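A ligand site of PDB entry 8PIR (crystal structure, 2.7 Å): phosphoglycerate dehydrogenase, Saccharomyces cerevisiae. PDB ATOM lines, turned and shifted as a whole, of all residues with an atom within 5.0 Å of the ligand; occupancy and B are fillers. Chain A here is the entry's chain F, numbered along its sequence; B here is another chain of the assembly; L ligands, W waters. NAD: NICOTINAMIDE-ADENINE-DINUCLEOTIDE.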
ATOM      1  N   ILE A 135     -20.545  18.243  10.085  1.00  0.00           N
ATOM      2  CA  ILE A 135     -20.828  18.333  11.547  1.00  0.00           C
ATOM      3  C   ILE A 135     -21.233  19.758  11.908  1.00  0.00           C
ATOM      4  O   ILE A 135     -22.135  19.915  12.734  1.00  0.00           O
ATOM      5  CB  ILE A 135     -19.588  17.907  12.350  1.00  0.00           C
ATOM      6  CG1 ILE A 135     -19.024  16.569  11.868  1.00  0.00           C
ATOM      7  CG2 ILE A 135     -19.861  17.899  13.839  1.00  0.00           C
ATOM      8  CD1 ILE A 135     -17.754  16.170  12.580  1.00  0.00           C
ATOM      9  N   PRO A 156     -23.380  14.625  12.893  1.00  0.00           N
ATOM     10  CA  PRO A 156     -22.309  14.898  13.837  1.00  0.00           C
ATOM     11  C   PRO A 156     -21.273  13.778  13.985  1.00  0.00           C
ATOM     12  O   PRO A 156     -20.146  14.095  14.298  1.00  0.00           O
ATOM     13  CB  PRO A 156     -23.050  15.122  15.174  1.00  0.00           C
ATOM     14  CG  PRO A 156     -24.378  14.400  14.996  1.00  0.00           C
ATOM     15  CD  PRO A 156     -24.696  14.485  13.526  1.00  0.00           C
ATOM     16  N   PHE A 157     -21.657  12.512  13.772  1.00  0.00           N
ATOM     17  CA  PHE A 157     -20.934  11.319  14.305  1.00  0.00           C
ATOM     18  C   PHE A 157     -20.565  10.327  13.190  1.00  0.00           C
ATOM     19  O   PHE A 157     -19.976   9.284  13.504  1.00  0.00           O
ATOM     20  CB  PHE A 157     -21.776  10.575  15.351  1.00  0.00           C
ATOM     21  CG  PHE A 157     -22.089  11.394  16.564  1.00  0.00           C
ATOM     22  CD1 PHE A 157     -21.107  12.147  17.186  1.00  0.00           C
ATOM     23  CD2 PHE A 157     -23.392  11.508  17.034  1.00  0.00           C
ATOM     24  CE1 PHE A 157     -21.405  12.947  18.279  1.00  0.00           C
ATOM     25  CE2 PHE A 157     -23.680  12.300  18.134  1.00  0.00           C
ATOM     26  CZ  PHE A 157     -22.694  13.032  18.744  1.00  0.00           C
ATOM     27  N   ASN A 159     -18.265  10.273  11.153  1.00  0.00           N
ATOM     28  CA  ASN A 159     -16.833  10.431  10.790  1.00  0.00           C
ATOM     29  C   ASN A 159     -15.934   9.651  11.759  1.00  0.00           C
ATOM     30  O   ASN A 159     -14.705   9.720  11.584  1.00  0.00           O
ATOM     31  CB  ASN A 159     -16.382  11.898  10.816  1.00  0.00           C
ATOM     32  CG  ASN A 159     -16.777  12.652   9.563  1.00  0.00           C
ATOM     33  OD1 ASN A 159     -17.375  12.082   8.651  1.00  0.00           O
ATOM     34  ND2 ASN A 159     -16.371  13.901   9.492  1.00  0.00           N
ATOM     35  N   VAL A 163     -11.626   8.723  11.687  1.00  0.00           N
ATOM     36  CA  VAL A 163     -10.661   9.413  12.605  1.00  0.00           C
ATOM     37  C   VAL A 163      -9.911   8.375  13.437  1.00  0.00           C
ATOM     38  O   VAL A 163      -8.693   8.579  13.660  1.00  0.00           O
ATOM     39  CB  VAL A 163     -11.385  10.439  13.501  1.00  0.00           C
ATOM     40  CG1 VAL A 163     -10.537  10.852  14.689  1.00  0.00           C
ATOM     41  CG2 VAL A 163     -11.803  11.666  12.717  1.00  0.00           C
ATOM     42  N   ILE A 208      -7.705  11.037  25.746  1.00  0.00           N
ATOM     43  CA  ILE A 208      -8.382  12.201  26.393  1.00  0.00           C
ATOM     44  C   ILE A 208      -9.696  12.462  25.645  1.00  0.00           C
ATOM     45  O   ILE A 208      -9.629  12.817  24.459  1.00  0.00           O
ATOM     46  CB  ILE A 208      -7.454  13.430  26.407  1.00  0.00           C
ATOM     47  CG1 ILE A 208      -6.171  13.155  27.181  1.00  0.00           C
ATOM     48  CG2 ILE A 208      -8.194  14.640  26.952  1.00  0.00           C
ATOM     49  CD1 ILE A 208      -5.042  14.103  26.855  1.00  0.00           C
ATOM     50  N   GLY A 209     -10.814  12.088  26.267  1.00  0.00           N
ATOM     51  CA  GLY A 209     -12.156  12.184  25.677  1.00  0.00           C
ATOM     52  C   GLY A 209     -12.606  10.853  25.126  1.00  0.00           C
ATOM     53  O   GLY A 209     -12.199  10.522  24.009  1.00  0.00           O
ATOM     54  N   TYR A 210     -13.390  10.102  25.906  1.00  0.00           N
ATOM     55  CA  TYR A 210     -13.844   8.726  25.597  1.00  0.00           C
ATOM     56  C   TYR A 210     -15.276   8.782  25.032  1.00  0.00           C
ATOM     57  O   TYR A 210     -16.149   8.035  25.488  1.00  0.00           O
ATOM     58  CB  TYR A 210     -13.759   7.867  26.853  1.00  0.00           C
ATOM     59  CG  TYR A 210     -13.602   6.384  26.593  1.00  0.00           C
ATOM     60  CD1 TYR A 210     -12.369   5.835  26.262  1.00  0.00           C
ATOM     61  CD2 TYR A 210     -14.660   5.521  26.789  1.00  0.00           C
ATOM     62  CE1 TYR A 210     -12.210   4.478  26.093  1.00  0.00           C
ATOM     63  CE2 TYR A 210     -14.512   4.150  26.622  1.00  0.00           C
ATOM     64  CZ  TYR A 210     -13.281   3.629  26.266  1.00  0.00           C
ATOM     65  OH  TYR A 210     -13.146   2.273  26.155  1.00  0.00           O
ATOM     66  N   GLY A 211     -15.463   9.600  23.987  1.00  0.00           N
ATOM     67  CA  GLY A 211     -16.753   9.781  23.305  1.00  0.00           C
ATOM     68  C   GLY A 211     -16.892   8.827  22.144  1.00  0.00           C
ATOM     69  O   GLY A 211     -16.429   7.678  22.251  1.00  0.00           O
ATOM     70  N   HIS A 212     -17.515   9.275  21.051  1.00  0.00           N
ATOM     71  CA  HIS A 212     -17.830   8.443  19.871  1.00  0.00           C
ATOM     72  C   HIS A 212     -16.537   7.908  19.263  1.00  0.00           C
ATOM     73  O   HIS A 212     -16.461   6.700  18.958  1.00  0.00           O
ATOM     74  CB  HIS A 212     -18.678   9.241  18.868  1.00  0.00           C
ATOM     75  CG  HIS A 212     -20.111   9.356  19.267  1.00  0.00           C
ATOM     76  ND1 HIS A 212     -20.564  10.267  20.212  1.00  0.00           N
ATOM     77  CD2 HIS A 212     -21.207   8.673  18.856  1.00  0.00           C
ATOM     78  CE1 HIS A 212     -21.872  10.143  20.341  1.00  0.00           C
ATOM     79  NE2 HIS A 212     -22.289   9.174  19.534  1.00  0.00           N
ATOM     80  N   ILE A 213     -15.545   8.790  19.104  1.00  0.00           N
ATOM     81  CA  ILE A 213     -14.243   8.481  18.460  1.00  0.00           C
ATOM     82  C   ILE A 213     -13.332   7.804  19.486  1.00  0.00           C
ATOM     83  O   ILE A 213     -12.722   6.794  19.152  1.00  0.00           O
ATOM     84  CB  ILE A 213     -13.587   9.741  17.879  1.00  0.00           C
ATOM     85  CG1 ILE A 213     -14.297  10.177  16.593  1.00  0.00           C
ATOM     86  CG2 ILE A 213     -12.101   9.523  17.647  1.00  0.00           C
ATOM     87  CD1 ILE A 213     -14.005  11.599  16.192  1.00  0.00           C
ATOM     88  N   GLY A 214     -13.167   8.423  20.653  1.00  0.00           N
ATOM     89  CA  GLY A 214     -12.396   7.847  21.768  1.00  0.00           C
ATOM     90  C   GLY A 214     -12.681   6.371  21.947  1.00  0.00           C
ATOM     91  O   GLY A 214     -11.710   5.582  22.056  1.00  0.00           O
ATOM     92  N   TYR A 231      -8.846   9.586  30.352  1.00  0.00           N
ATOM     93  CA  TYR A 231      -9.430  10.669  31.175  1.00  0.00           C
ATOM     94  C   TYR A 231     -10.664  11.232  30.468  1.00  0.00           C
ATOM     95  O   TYR A 231     -10.616  11.435  29.254  1.00  0.00           O
ATOM     96  CB  TYR A 231      -8.413  11.791  31.426  1.00  0.00           C
ATOM     97  CG  TYR A 231      -8.963  12.958  32.194  1.00  0.00           C
ATOM     98  CD1 TYR A 231      -9.340  12.833  33.518  1.00  0.00           C
ATOM     99  CD2 TYR A 231      -9.084  14.207  31.610  1.00  0.00           C
ATOM    100  CE1 TYR A 231      -9.843  13.903  34.238  1.00  0.00           C
ATOM    101  CE2 TYR A 231      -9.569  15.288  32.306  1.00  0.00           C
ATOM    102  CZ  TYR A 231      -9.970  15.136  33.621  1.00  0.00           C
ATOM    103  OH  TYR A 231     -10.446  16.210  34.325  1.00  0.00           O
ATOM    104  N   ASP A 232     -11.728  11.499  31.233  1.00  0.00           N
ATOM    105  CA  ASP A 232     -12.934  12.221  30.761  1.00  0.00           C
ATOM    106  C   ASP A 232     -13.561  12.943  31.962  1.00  0.00           C
ATOM    107  O   ASP A 232     -13.380  12.464  33.085  1.00  0.00           O
ATOM    108  CB  ASP A 232     -13.909  11.256  30.087  1.00  0.00           C
ATOM    109  CG  ASP A 232     -14.929  11.922  29.190  1.00  0.00           C
ATOM    110  OD1 ASP A 232     -15.581  12.873  29.641  1.00  0.00           O
ATOM    111  OD2 ASP A 232     -15.074  11.475  28.042  1.00  0.00           O
ATOM    112  N   ILE A 233     -14.177  14.103  31.727  1.00  0.00           N
ATOM    113  CA  ILE A 233     -14.793  14.946  32.790  1.00  0.00           C
ATOM    114  C   ILE A 233     -16.073  14.270  33.275  1.00  0.00           C
ATOM    115  O   ILE A 233     -16.654  14.740  34.256  1.00  0.00           O
ATOM    116  CB  ILE A 233     -15.044  16.382  32.298  1.00  0.00           C
ATOM    117  CG1 ILE A 233     -16.059  16.418  31.139  1.00  0.00           C
ATOM    118  CG2 ILE A 233     -13.744  17.076  31.923  1.00  0.00           C
ATOM    119  CD1 ILE A 233     -16.387  17.817  30.670  1.00  0.00           C
ATOM    120  N   VAL A 234     -16.457  13.163  32.642  1.00  0.00           N
ATOM    121  CA  VAL A 234     -17.630  12.336  33.033  1.00  0.00           C
ATOM    122  C   VAL A 234     -17.139  10.899  33.282  1.00  0.00           C
ATOM    123  O   VAL A 234     -16.193  10.479  32.602  1.00  0.00           O
ATOM    124  CB  VAL A 234     -18.713  12.373  31.935  1.00  0.00           C
ATOM    125  CG1 VAL A 234     -19.688  11.210  32.044  1.00  0.00           C
ATOM    126  CG2 VAL A 234     -19.449  13.710  31.956  1.00  0.00           C
ATOM    127  N   ILE A 236     -17.551   7.063  32.647  1.00  0.00           N
ATOM    128  CA  ILE A 236     -17.996   6.309  31.428  1.00  0.00           C
ATOM    129  C   ILE A 236     -17.565   4.847  31.585  1.00  0.00           C
ATOM    130  O   ILE A 236     -16.458   4.603  32.093  1.00  0.00           O
ATOM    131  CB  ILE A 236     -17.434   6.948  30.148  1.00  0.00           C
ATOM    132  CG1 ILE A 236     -17.726   8.444  30.086  1.00  0.00           C
ATOM    133  CG2 ILE A 236     -17.933   6.231  28.913  1.00  0.00           C
ATOM    134  CD1 ILE A 236     -16.851   9.206  29.121  1.00  0.00           C
ATOM    135  N   HIS A 261      -9.546  13.543  21.874  1.00  0.00           N
ATOM    136  CA  HIS A 261     -10.813  13.473  21.123  1.00  0.00           C
ATOM    137  C   HIS A 261     -11.825  14.235  21.949  1.00  0.00           C
ATOM    138  O   HIS A 261     -12.771  13.629  22.434  1.00  0.00           O
ATOM    139  CB  HIS A 261     -11.149  12.017  20.867  1.00  0.00           C
ATOM    140  CG  HIS A 261     -10.060  11.289  20.176  1.00  0.00           C
ATOM    141  ND1 HIS A 261      -9.720  11.551  18.871  1.00  0.00           N
ATOM    142  CD2 HIS A 261      -9.199  10.345  20.611  1.00  0.00           C
ATOM    143  CE1 HIS A 261      -8.716  10.790  18.525  1.00  0.00           C
ATOM    144  NE2 HIS A 261      -8.384  10.038  19.567  1.00  0.00           N
ATOM    145  N   VAL A 262     -11.608  15.538  22.117  1.00  0.00           N
ATOM    146  CA  VAL A 262     -12.432  16.347  23.040  1.00  0.00           C
ATOM    147  C   VAL A 262     -13.141  17.456  22.289  1.00  0.00           C
ATOM    148  O   VAL A 262     -12.692  17.813  21.216  1.00  0.00           O
ATOM    149  CB  VAL A 262     -11.544  16.907  24.157  1.00  0.00           C
ATOM    150  CG1 VAL A 262     -10.949  15.824  25.012  1.00  0.00           C
ATOM    151  CG2 VAL A 262     -10.471  17.826  23.610  1.00  0.00           C
ATOM    152  N   PRO A 263     -14.269  17.999  22.800  1.00  0.00           N
ATOM    153  CA  PRO A 263     -14.910  19.105  22.145  1.00  0.00           C
ATOM    154  C   PRO A 263     -14.153  20.400  22.375  1.00  0.00           C
ATOM    155  O   PRO A 263     -13.279  20.422  23.170  1.00  0.00           O
ATOM    156  CB  PRO A 263     -16.272  19.174  22.809  1.00  0.00           C
ATOM    157  CG  PRO A 263     -16.034  18.676  24.188  1.00  0.00           C
ATOM    158  CD  PRO A 263     -15.054  17.563  23.974  1.00  0.00           C
ATOM    159  N   ALA A 264     -14.481  21.433  21.610  1.00  0.00           N
ATOM    160  CA  ALA A 264     -13.886  22.760  21.824  1.00  0.00           C
ATOM    161  C   ALA A 264     -14.671  23.481  22.892  1.00  0.00           C
ATOM    162  O   ALA A 264     -15.823  23.808  22.654  1.00  0.00           O
ATOM    163  CB  ALA A 264     -13.894  23.532  20.546  1.00  0.00           C
ATOM    164  N   THR A 265     -14.075  23.625  24.066  1.00  0.00           N
ATOM    165  CA  THR A 265     -14.742  24.249  25.211  1.00  0.00           C
ATOM    166  C   THR A 265     -13.735  25.203  25.820  1.00  0.00           C
ATOM    167  O   THR A 265     -12.571  25.145  25.408  1.00  0.00           O
ATOM    168  CB  THR A 265     -15.133  23.188  26.257  1.00  0.00           C
ATOM    169  OG1 THR A 265     -13.980  22.762  26.972  1.00  0.00           O
ATOM    170  CG2 THR A 265     -15.882  22.012  25.690  1.00  0.00           C
ATOM    171  N   GLU A 267     -12.557  24.923  28.658  1.00  0.00           N
ATOM    172  CA  GLU A 267     -11.690  24.081  29.515  1.00  0.00           C
ATOM    173  C   GLU A 267     -10.792  23.176  28.672  1.00  0.00           C
ATOM    174  O   GLU A 267      -9.832  22.644  29.241  1.00  0.00           O
ATOM    175  CB  GLU A 267     -12.609  23.363  30.499  1.00  0.00           C
ATOM    176  CG  GLU A 267     -13.479  24.293  31.315  1.00  0.00           C
ATOM    177  CD  GLU A 267     -14.834  24.634  30.723  1.00  0.00           C
ATOM    178  OE1 GLU A 267     -15.163  24.070  29.659  1.00  0.00           O
ATOM    179  OE2 GLU A 267     -15.552  25.451  31.317  1.00  0.00           O
ATOM    180  N   THR A 268     -11.088  22.958  27.403  1.00  0.00           N
ATOM    181  CA  THR A 268     -10.212  22.202  26.464  1.00  0.00           C
ATOM    182  C   THR A 268      -9.189  23.138  25.810  1.00  0.00           C
ATOM    183  O   THR A 268      -8.133  22.647  25.361  1.00  0.00           O
ATOM    184  CB  THR A 268     -11.014  21.422  25.412  1.00  0.00           C
ATOM    185  OG1 THR A 268     -11.690  22.352  24.568  1.00  0.00           O
ATOM    186  CG2 THR A 268     -11.988  20.453  26.039  1.00  0.00           C
ATOM    187  N   MET A 271      -5.387  22.838  26.587  1.00  0.00           N
ATOM    188  CA  MET A 271      -5.384  21.963  27.786  1.00  0.00           C
ATOM    189  C   MET A 271      -4.108  21.114  27.820  1.00  0.00           C
ATOM    190  O   MET A 271      -3.693  20.721  28.925  1.00  0.00           O
ATOM    191  CB  MET A 271      -6.621  21.061  27.841  1.00  0.00           C
ATOM    192  CG  MET A 271      -6.585  19.874  26.899  1.00  0.00           C
ATOM    193  SD  MET A 271      -8.125  18.886  26.926  1.00  0.00           S
ATOM    194  CE  MET A 271      -8.057  18.149  28.560  1.00  0.00           C
ATOM    195  N   ALA A 289      -6.191  15.045  16.495  1.00  0.00           N
ATOM    196  CA  ALA A 289      -7.204  15.101  15.419  1.00  0.00           C
ATOM    197  C   ALA A 289      -8.561  15.555  15.991  1.00  0.00           C
ATOM    198  O   ALA A 289      -9.585  15.206  15.369  1.00  0.00           O
ATOM    199  CB  ALA A 289      -7.299  13.740  14.758  1.00  0.00           C
ATOM    200  N   SER A 290      -8.567  16.350  17.067  1.00  0.00           N
ATOM    201  CA  SER A 290      -9.799  16.912  17.689  1.00  0.00           C
ATOM    202  C   SER A 290     -10.085  18.324  17.152  1.00  0.00           C
ATOM    203  O   SER A 290     -10.740  18.417  16.093  1.00  0.00           O
ATOM    204  CB  SER A 290      -9.749  16.902  19.201  1.00  0.00           C
ATOM    205  OG  SER A 290      -8.728  17.753  19.695  1.00  0.00           O
ATOM    206  N   ARG A 291      -9.601  19.368  17.838  1.00  0.00           N
ATOM    207  CA  ARG A 291      -9.872  20.797  17.511  1.00  0.00           C
ATOM    208  C   ARG A 291      -8.558  21.596  17.487  1.00  0.00           C
ATOM    209  O   ARG A 291      -7.684  21.325  18.334  1.00  0.00           O
ATOM    210  CB  ARG A 291     -10.837  21.395  18.520  1.00  0.00           C
ATOM    211  CG  ARG A 291     -12.238  20.813  18.464  1.00  0.00           C
ATOM    212  CD  ARG A 291     -12.889  20.998  17.115  1.00  0.00           C
ATOM    213  NE  ARG A 291     -14.280  20.546  17.171  1.00  0.00           N
ATOM    214  CZ  ARG A 291     -15.336  21.337  17.174  1.00  0.00           C
ATOM    215  NH1 ARG A 291     -15.194  22.644  17.082  1.00  0.00           N
ATOM    216  NH2 ARG A 291     -16.547  20.824  17.219  1.00  0.00           N
ATOM    217  N   ASP A 315      -3.794  17.150  12.880  1.00  0.00           N
ATOM    218  CA  ASP A 315      -4.772  17.201  11.767  1.00  0.00           C
ATOM    219  C   ASP A 315      -5.461  18.575  11.751  1.00  0.00           C
ATOM    220  O   ASP A 315      -6.144  18.876  10.753  1.00  0.00           O
ATOM    221  CB  ASP A 315      -5.797  16.068  11.889  1.00  0.00           C
ATOM    222  CG  ASP A 315      -6.602  15.841  10.609  1.00  0.00           C
ATOM    223  OD1 ASP A 315      -5.988  15.883   9.517  1.00  0.00           O
ATOM    224  OD2 ASP A 315      -7.821  15.613  10.726  1.00  0.00           O
ATOM    225  N   VAL A 316      -5.370  19.257  12.900  1.00  0.00           N
ATOM    226  CA  VAL A 316      -6.139  20.507  13.134  1.00  0.00           C
ATOM    227  C   VAL A 316      -5.233  21.597  13.696  1.00  0.00           C
ATOM    228  O   VAL A 316      -4.299  21.244  14.429  1.00  0.00           O
ATOM    229  CB  VAL A 316      -7.294  20.163  14.083  1.00  0.00           C
ATOM    230  CG1 VAL A 316      -8.261  19.185  13.453  1.00  0.00           C
ATOM    231  CG2 VAL A 316      -6.784  19.630  15.400  1.00  0.00           C
ATOM    232  N   HIS A 351      -6.724  18.555   7.922  1.00  0.00           N
ATOM    233  CA  HIS A 351      -8.114  18.281   8.362  1.00  0.00           C
ATOM    234  C   HIS A 351      -8.709  17.135   7.560  1.00  0.00           C
ATOM    235  O   HIS A 351      -9.830  17.268   7.095  1.00  0.00           O
ATOM    236  CB  HIS A 351      -8.976  19.553   8.348  1.00  0.00           C
ATOM    237  CG  HIS A 351      -9.970  19.617   9.456  1.00  0.00           C
ATOM    238  ND1 HIS A 351     -10.211  20.778  10.156  1.00  0.00           N
ATOM    239  CD2 HIS A 351     -10.770  18.680   9.997  1.00  0.00           C
ATOM    240  CE1 HIS A 351     -11.128  20.559  11.067  1.00  0.00           C
ATOM    241  NE2 HIS A 351     -11.483  19.286  10.996  1.00  0.00           N
ATOM    242  N   ILE A 352      -8.001  16.024   7.483  1.00  0.00           N
ATOM    243  CA  ILE A 352      -8.495  14.879   6.661  1.00  0.00           C
ATOM    244  C   ILE A 352      -9.001  13.754   7.565  1.00  0.00           C
ATOM    245  O   ILE A 352      -9.423  12.721   7.024  1.00  0.00           O
ATOM    246  CB  ILE A 352      -7.424  14.372   5.684  1.00  0.00           C
ATOM    247  CG1 ILE A 352      -6.179  13.866   6.419  1.00  0.00           C
ATOM    248  CG2 ILE A 352      -7.071  15.446   4.660  1.00  0.00           C
ATOM    249  CD1 ILE A 352      -5.196  13.171   5.522  1.00  0.00           C
ATOM    250  N   GLY A 353      -9.118  14.010   8.868  1.00  0.00           N
ATOM    251  CA  GLY A 353      -9.696  13.075   9.859  1.00  0.00           C
ATOM    252  C   GLY A 353     -10.875  12.294   9.316  1.00  0.00           C
ATOM    253  O   GLY A 353     -10.894  11.059   9.505  1.00  0.00           O
ATOM    254  N   GLY A 354     -11.858  12.985   8.742  1.00  0.00           N
ATOM    255  CA  GLY A 354     -13.113  12.386   8.230  1.00  0.00           C
ATOM    256  C   GLY A 354     -13.115  12.253   6.719  1.00  0.00           C
ATOM    257  O   GLY A 354     -14.193  12.001   6.151  1.00  0.00           O
ATOM    258  N   ARG B  45     -22.605   6.367  29.881  1.00  0.00           N
ATOM    259  CA  ARG B  45     -21.972   7.502  30.596  1.00  0.00           C
ATOM    260  C   ARG B  45     -22.921   7.971  31.699  1.00  0.00           C
ATOM    261  O   ARG B  45     -24.122   8.085  31.427  1.00  0.00           O
ATOM    262  CB  ARG B  45     -21.620   8.635  29.628  1.00  0.00           C
ATOM    263  CG  ARG B  45     -22.734   8.979  28.650  1.00  0.00           C
ATOM    264  CD  ARG B  45     -22.314  10.077  27.697  1.00  0.00           C
ATOM    265  NE  ARG B  45     -21.025   9.780  27.095  1.00  0.00           N
ATOM    266  CZ  ARG B  45     -19.919  10.508  27.242  1.00  0.00           C
ATOM    267  NH1 ARG B  45     -19.943  11.620  27.963  1.00  0.00           N
ATOM    268  NH2 ARG B  45     -18.800  10.112  26.684  1.00  0.00           N
HETATM  269  PA  NAD L   1     -18.020  13.298  21.532  1.00  0.00           P
HETATM  270  O1A NAD L   1     -18.926  14.359  21.948  1.00  0.00           O
HETATM  271  O2A NAD L   1     -18.606  11.885  21.278  1.00  0.00           O
HETATM  272  O5B NAD L   1     -16.880  13.017  22.643  1.00  0.00           O
HETATM  273  C5B NAD L   1     -16.238  14.098  23.322  1.00  0.00           C
HETATM  274  C4B NAD L   1     -15.827  13.566  24.674  1.00  0.00           C
HETATM  275  O4B NAD L   1     -15.021  14.561  25.340  1.00  0.00           O
HETATM  276  C3B NAD L   1     -16.992  13.240  25.628  1.00  0.00           C
HETATM  277  O3B NAD L   1     -16.826  11.935  26.166  1.00  0.00           O
HETATM  278  C2B NAD L   1     -16.871  14.336  26.707  1.00  0.00           C
HETATM  279  O2B NAD L   1     -17.265  13.925  28.005  1.00  0.00           O
HETATM  280  C1B NAD L   1     -15.374  14.540  26.706  1.00  0.00           C
HETATM  281  N9A NAD L   1     -14.910  15.769  27.326  1.00  0.00           N
HETATM  282  C8A NAD L   1     -15.426  17.036  27.186  1.00  0.00           C
HETATM  283  N7A NAD L   1     -14.682  17.971  27.728  1.00  0.00           N
HETATM  284  C5A NAD L   1     -13.614  17.276  28.268  1.00  0.00           C
HETATM  285  C6A NAD L   1     -12.401  17.707  28.848  1.00  0.00           C
HETATM  286  N6A NAD L   1     -12.030  18.991  28.895  1.00  0.00           N
HETATM  287  N1A NAD L   1     -11.489  16.772  29.157  1.00  0.00           N
HETATM  288  C2A NAD L   1     -11.746  15.495  28.852  1.00  0.00           C
HETATM  289  N3A NAD L   1     -12.836  14.981  28.291  1.00  0.00           N
HETATM  290  C4A NAD L   1     -13.746  15.924  28.037  1.00  0.00           C
HETATM  291  O3  NAD L   1     -17.171  13.770  20.270  1.00  0.00           O
HETATM  292  PN  NAD L   1     -16.652  12.904  19.030  1.00  0.00           P
HETATM  293  O1N NAD L   1     -17.810  12.798  18.106  1.00  0.00           O
HETATM  294  O2N NAD L   1     -16.045  11.671  19.554  1.00  0.00           O
HETATM  295  O5D NAD L   1     -15.511  13.840  18.398  1.00  0.00           O
HETATM  296  C5D NAD L   1     -14.403  14.315  19.221  1.00  0.00           C
HETATM  297  C4D NAD L   1     -13.816  15.621  18.731  1.00  0.00           C
HETATM  298  O4D NAD L   1     -13.152  15.437  17.451  1.00  0.00           O
HETATM  299  C3D NAD L   1     -14.803  16.755  18.507  1.00  0.00           C
HETATM  300  O3D NAD L   1     -14.170  18.005  18.786  1.00  0.00           O
HETATM  301  C2D NAD L   1     -15.092  16.637  17.004  1.00  0.00           C
HETATM  302  O2D NAD L   1     -15.580  17.840  16.434  1.00  0.00           O
HETATM  303  C1D NAD L   1     -13.692  16.304  16.492  1.00  0.00           C
HETATM  304  N1N NAD L   1     -13.680  15.634  15.143  1.00  0.00           N
HETATM  305  C2N NAD L   1     -12.731  16.008  14.259  1.00  0.00           C
HETATM  306  C3N NAD L   1     -12.735  15.497  12.976  1.00  0.00           C
HETATM  307  C7N NAD L   1     -11.533  15.665  12.104  1.00  0.00           C
HETATM  308  O7N NAD L   1     -11.665  15.670  10.890  1.00  0.00           O
HETATM  309  N7N NAD L   1     -10.349  15.812  12.700  1.00  0.00           N
HETATM  310  C4N NAD L   1     -13.786  14.662  12.589  1.00  0.00           C
HETATM  311  C5N NAD L   1     -14.737  14.282  13.524  1.00  0.00           C
HETATM  312  C6N NAD L   1     -14.652  14.763  14.821  1.00  0.00           C
HETATM  313  O   HOH W   1     -14.390  11.188  21.425  1.00  0.00           O
HETATM  314  O   HOH W   2     -17.659  18.353  18.213  1.00  0.00           O
HETATM  315  O   HOH W   3     -11.220  13.381  17.224  1.00  0.00           O
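The side-chain carboxylate (OD1) of Asp 232 is in hydrogen-bond range of an oxygen (O2B) of the ligand.
N of Gly 211 sits at hydrogen-bond distance from O3B of the ligand (3.5 Å).
An oxygen (O3D) of the ligand is in hydrogen-bond range of the guanidinium group (NE) of Arg 291 (3.0 Å).
O2A of the ligand is in hydrogen-bond range of ND1 of His 212 (2.8 Å).
OD2 of Asp 315 sits at hydrogen-bond distance from N7N of the ligand, 3.2 Å away.
O2N of the ligand is in hydrogen-bond range of N of Ile 213, 3.0 Å away.
O2A of the ligand sits at hydrogen-bond distance from N of His 212, at 2.8 Å.
N of Gly 354 is in hydrogen-bond range of O7N of the ligand (3.4 Å).
A nitrogen (N7N) of the ligand lies within hydrogen-bond range of the backbone carbonyl oxygen of Ala 289 (2.8 Å).
O of Val 262 lies within hydrogen-bond range of O3D of the ligand, 2.9 Å away.
The guanidinium group of Arg 45 of chain B is in hydrogen-bond range of an oxygen (O3B) of the ligand.
N of His 261 lies within hydrogen-bond range of O of Ile 208 (2.7 Å).
The backbone NH (N) of Tyr 210 lies within hydrogen-bond range of the side-chain carboxylate (OD2) of Asp 232 (3.0 Å).
OG1 of Thr 268 lies within hydrogen-bond range of N of Thr 265 (2.7 Å).
The backbone carbonyl oxygen (O) of Gly 353 sits at hydrogen-bond distance from the backbone NH (N) of Val 163, at 3.3 Å.
N of Ile 352 is in hydrogen-bond range of OD1 of Asp 315 (2.9 Å).
N of His 351 sits at hydrogen-bond distance from O of Asp 315 (2.9 Å).
The side-chain carboxylate (OD1) of Asp 232 sits close to the backbone NH (N) of Val 234, at 3.1 Å.
The backbone NH (N) of Gly 209 sits at hydrogen-bond distance from the backbone carbonyl oxygen (O) of Tyr 231, 3.1 Å away.
Ile 135 touches the ligand (CD1 to C5N, 3.7 Å).
Phe 157 touches the ligand.
Asn 159 touches the ligand.
CG2 of Val 163 touches C4N of the ligand, 3.6 Å away.
CA of Gly 209 touches O4B of the ligand (3.7 Å).
Tyr 210 touches the ligand.
Tyr 231 touches the ligand.
Ile 233 touches the ligand.
His 261 touches the ligand (O to C5B, 3.6 Å).
CD of Pro 263 touches C8A of the ligand, 3.3 Å away.
Thr 268 touches the ligand (CG2 to N6A, 3.2 Å).
Met 271 touches the ligand (CE to N1A, 3.7 Å).
Ser 290 touches the ligand.
His 351 touches the ligand.
CA of Gly 353 touches O7N of the ligand, at 3.4 Å.
Hydrophobic or aromatic side chains that line the ligand: Ile 135, Phe 157, Val 163, His 212, Ile 213, Tyr 231, Ile 233, Val 262, Pro 263, Met 271 and His 351.
Within 4 Å of the ligand: Ile 135, Phe 157, Asn 159, Val 163, Gly 209, Tyr 210, Gly 211, His 212, Ile 213, Tyr 231, Asp 232, Ile 233, His 261, Val 262, Pro 263, Thr 268, Met 271, Ala 289, Ser 290, Arg 291, Asp 315, His 351, Gly 353, Gly 354 and Arg 45 of chain B.
The nearest printed residue that does not touch the ligand is Ile 236 (4.02 Å).
Water W1 lies within hydrogen-bond range of an oxygen (O2N) of the ligand, the backbone carbonyl oxygen (O) of His 261, the backbone NH (N) of Gly 214, the backbone NH (N) of Gly 211 and the backbone carbonyl oxygen (O) of Gly 209.
Water W2 bridges O2D of the ligand (2.8 Å) and NH2 of Arg 291 (2.9 Å).
Water W3 lies within hydrogen-bond range of O4D of the ligand (2.8 Å), ND1 of His 261 (2.9 Å) and O of Ala 289 (3.1 Å).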
